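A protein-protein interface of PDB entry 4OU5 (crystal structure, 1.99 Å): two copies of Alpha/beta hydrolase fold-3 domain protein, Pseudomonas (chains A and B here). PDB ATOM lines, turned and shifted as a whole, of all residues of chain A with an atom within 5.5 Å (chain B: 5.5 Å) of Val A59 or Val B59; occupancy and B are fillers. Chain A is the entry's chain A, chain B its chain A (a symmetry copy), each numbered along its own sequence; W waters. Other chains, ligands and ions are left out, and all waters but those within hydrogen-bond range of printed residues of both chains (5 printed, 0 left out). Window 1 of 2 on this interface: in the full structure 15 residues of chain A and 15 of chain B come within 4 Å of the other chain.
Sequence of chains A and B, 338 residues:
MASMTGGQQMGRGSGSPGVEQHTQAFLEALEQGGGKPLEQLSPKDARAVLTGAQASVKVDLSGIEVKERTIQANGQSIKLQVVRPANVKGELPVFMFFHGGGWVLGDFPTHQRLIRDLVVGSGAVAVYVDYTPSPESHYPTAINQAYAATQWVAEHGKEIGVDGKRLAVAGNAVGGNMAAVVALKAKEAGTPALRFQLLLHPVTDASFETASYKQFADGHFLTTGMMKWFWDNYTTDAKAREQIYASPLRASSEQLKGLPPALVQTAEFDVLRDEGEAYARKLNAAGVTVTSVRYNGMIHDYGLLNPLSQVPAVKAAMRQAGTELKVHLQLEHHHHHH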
ATOM      1  N   VAL A  57       3.512  15.773 -16.386  1.00  0.00           N
ATOM      2  CA  VAL A  57       3.098  17.118 -16.024  1.00  0.00           C
ATOM      3  C   VAL A  57       2.645  17.884 -17.264  1.00  0.00           C
ATOM      4  O   VAL A  57       3.379  17.977 -18.243  1.00  0.00           O
ATOM      5  CB  VAL A  57       4.257  17.899 -15.336  1.00  0.00           C
ATOM      6  CG1 VAL A  57       3.760  19.234 -14.815  1.00  0.00           C
ATOM      7  CG2 VAL A  57       4.865  17.074 -14.204  1.00  0.00           C
ATOM      8  N   LYS A  58       1.434  18.418 -17.235  1.00  0.00           N
ATOM      9  CA  LYS A  58       0.980  19.277 -18.318  1.00  0.00           C
ATOM     10  C   LYS A  58       1.809  20.571 -18.318  1.00  0.00           C
ATOM     11  O   LYS A  58       1.848  21.275 -17.311  1.00  0.00           O
ATOM     12  CB  LYS A  58      -0.513  19.578 -18.163  1.00  0.00           C
ATOM     13  CG  LYS A  58      -1.086  20.436 -19.258  1.00  0.00           C
ATOM     14  CD  LYS A  58      -2.546  20.795 -18.975  1.00  0.00           C
ATOM     15  CE  LYS A  58      -2.642  21.938 -17.982  1.00  0.00           C
ATOM     16  NZ  LYS A  58      -4.009  22.534 -17.954  1.00  0.00           N
ATOM     17  N   VAL A  59       2.494  20.863 -19.425  1.00  0.00           N
ATOM     18  CA  VAL A  59       3.320  22.068 -19.510  1.00  0.00           C
ATOM     19  C   VAL A  59       3.133  22.799 -20.838  1.00  0.00           C
ATOM     20  O   VAL A  59       2.824  22.192 -21.865  1.00  0.00           O
ATOM     21  CB  VAL A  59       4.839  21.763 -19.325  1.00  0.00           C
ATOM     22  CG1 VAL A  59       5.125  21.225 -17.920  1.00  0.00           C
ATOM     23  CG2 VAL A  59       5.349  20.793 -20.401  1.00  0.00           C
ATOM     24  N   ASP A  60       3.330  24.113 -20.801  1.00  0.00           N
ATOM     25  CA  ASP A  60       3.243  24.968 -21.982  1.00  0.00           C
ATOM     26  C   ASP A  60       4.545  24.896 -22.796  1.00  0.00           C
ATOM     27  O   ASP A  60       5.604  25.333 -22.331  1.00  0.00           O
ATOM     28  CB  ASP A  60       2.941  26.408 -21.547  1.00  0.00           C
ATOM     29  CG  ASP A  60       2.678  27.352 -22.716  1.00  0.00           C
ATOM     30  OD1 ASP A  60       2.641  26.919 -23.886  1.00  0.00           O
ATOM     31  OD2 ASP A  60       2.498  28.554 -22.444  1.00  0.00           O
ATOM     32  N   LEU A  61       4.457  24.330 -24.000  1.00  0.00           N
ATOM     33  CA  LEU A  61       5.600  24.244 -24.915  1.00  0.00           C
ATOM     34  C   LEU A  61       5.387  25.089 -26.165  1.00  0.00           C
ATOM     35  O   LEU A  61       6.130  24.958 -27.135  1.00  0.00           O
ATOM     36  CB  LEU A  61       5.862  22.789 -25.323  1.00  0.00           C
ATOM     37  CG  LEU A  61       6.191  21.815 -24.178  1.00  0.00           C
ATOM     38  CD1 LEU A  61       6.429  20.420 -24.711  1.00  0.00           C
ATOM     39  CD2 LEU A  61       7.415  22.295 -23.427  1.00  0.00           C
ATOM     40  N   SER A  62       4.378  25.952 -26.144  1.00  0.00           N
ATOM     41  CA  SER A  62       4.058  26.794 -27.297  1.00  0.00           C
ATOM     42  C   SER A  62       5.092  27.883 -27.548  1.00  0.00           C
ATOM     43  O   SER A  62       5.935  28.166 -26.691  1.00  0.00           O
ATOM     44  CB  SER A  62       2.690  27.451 -27.115  1.00  0.00           C
ATOM     45  OG  SER A  62       2.714  28.347 -26.021  1.00  0.00           O
ATOM     46  N   ARG A 113      10.966  21.609 -21.987  1.00  0.00           N
ATOM     47  CA  ARG A 113      10.216  22.717 -21.384  1.00  0.00           C
ATOM     48  C   ARG A 113      11.169  23.833 -20.919  1.00  0.00           C
ATOM     49  O   ARG A 113      10.902  25.018 -21.115  1.00  0.00           O
ATOM     50  CB  ARG A 113       9.349  22.240 -20.211  1.00  0.00           C
ATOM     51  CG  ARG A 113       8.259  23.261 -19.816  1.00  0.00           C
ATOM     52  CD  ARG A 113       8.292  23.587 -18.331  1.00  0.00           C
ATOM     53  NE  ARG A 113       9.328  24.572 -18.015  1.00  0.00           N
ATOM     54  CZ  ARG A 113      10.384  24.331 -17.245  1.00  0.00           C
ATOM     55  NH1 ARG A 113      11.269  25.294 -17.023  1.00  0.00           N
ATOM     56  NH2 ARG A 113      10.561  23.134 -16.697  1.00  0.00           N
ATOM     57  N   ASN A 306       9.716  19.536 -14.271  1.00  0.00           N
ATOM     58  CA  ASN A 306       8.432  20.074 -14.682  1.00  0.00           C
ATOM     59  C   ASN A 306       7.417  20.233 -13.532  1.00  0.00           C
ATOM     60  O   ASN A 306       6.622  21.168 -13.565  1.00  0.00           O
ATOM     61  CB  ASN A 306       7.860  19.232 -15.823  1.00  0.00           C
ATOM     62  CG  ASN A 306       8.599  19.475 -17.119  1.00  0.00           C
ATOM     63  OD1 ASN A 306       9.364  20.445 -17.229  1.00  0.00           O
ATOM     64  ND2 ASN A 306       8.390  18.610 -18.107  1.00  0.00           N
ATOM     65  N   SER A 309       7.703  23.817 -12.406  1.00  0.00           N
ATOM     66  CA  SER A 309       7.805  24.840 -13.441  1.00  0.00           C
ATOM     67  C   SER A 309       6.831  26.002 -13.263  1.00  0.00           C
ATOM     68  O   SER A 309       6.995  27.037 -13.911  1.00  0.00           O
ATOM     69  CB  SER A 309       7.606  24.222 -14.832  1.00  0.00           C
ATOM     70  OG  SER A 309       6.285  23.742 -14.991  1.00  0.00           O
ATOM     71  N   VAL B  57      -0.382  28.192 -29.958  1.00  0.00           N
ATOM     72  CA  VAL B  57      -1.444  27.749 -29.072  1.00  0.00           C
ATOM     73  C   VAL B  57      -0.869  26.907 -27.935  1.00  0.00           C
ATOM     74  O   VAL B  57      -0.161  25.934 -28.175  1.00  0.00           O
ATOM     75  CB  VAL B  57      -2.507  26.909 -29.841  1.00  0.00           C
ATOM     76  CG1 VAL B  57      -3.690  26.599 -28.942  1.00  0.00           C
ATOM     77  CG2 VAL B  57      -2.968  27.643 -31.098  1.00  0.00           C
ATOM     78  N   LYS B  58      -1.153  27.287 -26.700  1.00  0.00           N
ATOM     79  CA  LYS B  58      -0.760  26.465 -25.566  1.00  0.00           C
ATOM     80  C   LYS B  58      -1.552  25.148 -25.596  1.00  0.00           C
ATOM     81  O   LYS B  58      -2.780  25.171 -25.597  1.00  0.00           O
ATOM     82  CB  LYS B  58      -0.998  27.221 -24.257  1.00  0.00           C
ATOM     83  CG  LYS B  58      -0.588  26.463 -23.023  1.00  0.00           C
ATOM     84  CD  LYS B  58      -0.965  27.227 -21.751  1.00  0.00           C
ATOM     85  CE  LYS B  58      -2.435  27.039 -21.421  1.00  0.00           C
ATOM     86  NZ  LYS B  58      -2.748  27.470 -20.028  1.00  0.00           N
ATOM     87  N   VAL B  59      -0.855  24.012 -25.658  1.00  0.00           N
ATOM     88  CA  VAL B  59      -1.526  22.712 -25.704  1.00  0.00           C
ATOM     89  C   VAL B  59      -0.870  21.695 -24.773  1.00  0.00           C
ATOM     90  O   VAL B  59       0.330  21.757 -24.500  1.00  0.00           O
ATOM     91  CB  VAL B  59      -1.562  22.111 -27.144  1.00  0.00           C
ATOM     92  CG1 VAL B  59      -2.397  22.985 -28.084  1.00  0.00           C
ATOM     93  CG2 VAL B  59      -0.145  21.904 -27.698  1.00  0.00           C
ATOM     94  N   ASP B  60      -1.677  20.754 -24.294  1.00  0.00           N
ATOM     95  CA  ASP B  60      -1.217  19.671 -23.429  1.00  0.00           C
ATOM     96  C   ASP B  60      -0.570  18.552 -24.263  1.00  0.00           C
ATOM     97  O   ASP B  60      -1.247  17.882 -25.051  1.00  0.00           O
ATOM     98  CB  ASP B  60      -2.398  19.137 -22.608  1.00  0.00           C
ATOM     99  CG  ASP B  60      -1.993  18.106 -21.560  1.00  0.00           C
ATOM    100  OD1 ASP B  60      -0.790  17.827 -21.376  1.00  0.00           O
ATOM    101  OD2 ASP B  60      -2.909  17.573 -20.905  1.00  0.00           O
ATOM    102  N   LEU B  61       0.739  18.372 -24.092  1.00  0.00           N
ATOM    103  CA  LEU B  61       1.482  17.306 -24.772  1.00  0.00           C
ATOM    104  C   LEU B  61       2.010  16.269 -23.788  1.00  0.00           C
ATOM    105  O   LEU B  61       2.840  15.438 -24.150  1.00  0.00           O
ATOM    106  CB  LEU B  61       2.652  17.886 -25.576  1.00  0.00           C
ATOM    107  CG  LEU B  61       2.281  18.886 -26.685  1.00  0.00           C
ATOM    108  CD1 LEU B  61       3.518  19.380 -27.400  1.00  0.00           C
ATOM    109  CD2 LEU B  61       1.340  18.233 -27.676  1.00  0.00           C
ATOM    110  N   SER B  62       1.530  16.316 -22.550  1.00  0.00           N
ATOM    111  CA  SER B  62       1.986  15.391 -21.512  1.00  0.00           C
ATOM    112  C   SER B  62       1.508  13.962 -21.732  1.00  0.00           C
ATOM    113  O   SER B  62       0.612  13.711 -22.544  1.00  0.00           O
ATOM    114  CB  SER B  62       1.512  15.859 -20.137  1.00  0.00           C
ATOM    115  OG  SER B  62       0.100  15.810 -20.057  1.00  0.00           O
ATOM    116  N   ARG B 113       0.425  17.309 -31.344  1.00  0.00           N
ATOM    117  CA  ARG B 113      -0.681  17.334 -30.378  1.00  0.00           C
ATOM    118  C   ARG B 113      -1.750  16.290 -30.745  1.00  0.00           C
ATOM    119  O   ARG B 113      -2.274  15.587 -29.881  1.00  0.00           O
ATOM    120  CB  ARG B 113      -1.315  18.729 -30.282  1.00  0.00           C
ATOM    121  CG  ARG B 113      -2.186  18.906 -29.018  1.00  0.00           C
ATOM    122  CD  ARG B 113      -3.580  19.411 -29.352  1.00  0.00           C
ATOM    123  NE  ARG B 113      -4.457  18.329 -29.803  1.00  0.00           N
ATOM    124  CZ  ARG B 113      -4.984  18.247 -31.020  1.00  0.00           C
ATOM    125  NH1 ARG B 113      -5.765  17.220 -31.329  1.00  0.00           N
ATOM    126  NH2 ARG B 113      -4.735  19.183 -31.928  1.00  0.00           N
ATOM    127  N   ASN B 306      -4.559  23.190 -33.788  1.00  0.00           N
ATOM    128  CA  ASN B 306      -4.487  23.392 -32.352  1.00  0.00           C
ATOM    129  C   ASN B 306      -5.468  24.453 -31.813  1.00  0.00           C
ATOM    130  O   ASN B 306      -5.955  24.301 -30.697  1.00  0.00           O
ATOM    131  CB  ASN B 306      -3.046  23.703 -31.946  1.00  0.00           C
ATOM    132  CG  ASN B 306      -2.170  22.474 -32.016  1.00  0.00           C
ATOM    133  OD1 ASN B 306      -2.680  21.348 -32.121  1.00  0.00           O
ATOM    134  ND2 ASN B 306      -0.855  22.663 -31.964  1.00  0.00           N
ATOM    135  N   SER B 309      -8.489  22.540 -30.626  1.00  0.00           N
ATOM    136  CA  SER B 309      -8.253  21.310 -29.877  1.00  0.00           C
ATOM    137  C   SER B 309      -9.036  21.221 -28.569  1.00  0.00           C
ATOM    138  O   SER B 309      -9.123  20.139 -27.985  1.00  0.00           O
ATOM    139  CB  SER B 309      -6.757  21.135 -29.583  1.00  0.00           C
ATOM    140  OG  SER B 309      -6.291  22.138 -28.701  1.00  0.00           O
HETATM  141  O   HOH W   1      -2.224  25.219 -18.441  1.00  0.00           O
HETATM  142  O   HOH W   2      -0.437  23.205 -21.479  1.00  0.00           O
HETATM  143  O   HOH W   3       2.590  19.542 -22.123  1.00  0.00           O
HETATM  144  O   HOH W   4       2.099  23.470 -25.540  1.00  0.00           O
HETATM  145  O   HOH W   5      -4.000  24.460 -19.991  1.00  0.00           O
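The side-chain carboxylate of Asp B60 is in hydrogen-bond range of the side-chain hydroxyl of Ser B62, at 2.6 Å. OD1 of Asp A60 sits at hydrogen-bond distance from OG of Ser A62.
Of the 9 printed residues of chain B, 5 touch a printed residue of chain A. Printed residues of chain A that touch a printed residue of chain B: Val A57, Lys A58, Val A59, Asp A60 and Ser A62. Among the printed residues, 7 pairs touch across the chains. Among the printed residues, no Asp or Glu carboxylate lies within 4 Å of a Lys or Arg side-chain nitrogen of the other chain.
Val A57 touches Ser B62, and with the chains exchanged Ser A62 touches Val B57. Lys A58 touches Asp B60, and with the chains exchanged Asp A60 touches Lys B58. Lys A58 touches Ser B62, and with the chains exchanged Ser A62 touches Lys B58. Val A59 touches its own counterpart, Val B59. 9 positions are printed for both chains. Of the 7 pairs that touch across the chains among the printed residues, 7 have their exchanged pair printed and touching as well.
Of chain B, only Val B59 (3.7 Å) comes within 4 Å of Val A59. Of chain A, only Val A59 (3.7 Å) comes within 4 Å of Val B59. Of the printed residues of chain A, Asp B60 touches Lys A58. Of the printed residues of chain B, Asp A60 touches Lys B58. Printed residues of chain B within 4 Å of Ser A62: Val B57 and Lys B58. Of the printed residues of chain A, Val B57 touches Ser A62. Ser B309 touches none of the printed residues of chain A. The nearest printed residue of chain A that does not touch Val B59 is Asp A60 (4.9 Å).
Water W3 lies within hydrogen-bond range of the backbone carbonyl oxygen (O) of Val A59 (2.7 Å), the backbone NH (N) of Leu B61 (2.9 Å) and the backbone NH (N) of Ser B62 (3.4 Å). Water W4 lies within hydrogen-bond range of the backbone carbonyl oxygen of Val B59, the backbone NH of Leu A61 and the backbone NH of Ser A62. Water W5 lies within hydrogen-bond range of the side-chain amino group of Lys A58 and the side-chain amino group of Lys B58. Water W1 bridges the side-chain amino group of Lys B58 (2.8 Å) and the side-chain amino group of Lys A58 (3.3 Å). Water W2 lies within hydrogen-bond range of the backbone carbonyl oxygen (O) of Val B59 and the backbone carbonyl oxygen (O) of Val A59.
O of Val A57 touches CB of Ser B62, at 3.4 Å. Lys A58 touches Asp B60. Lys A58 touches Ser B62. O of Val A59 touches O of Val B59, 3.7 Å away. Asp A60 touches Lys B58. Ser A62 touches Val B57 (CB to O, 3.4 Å). N of Lys B58 touches CB of Ser A62, at 3.9 Å.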
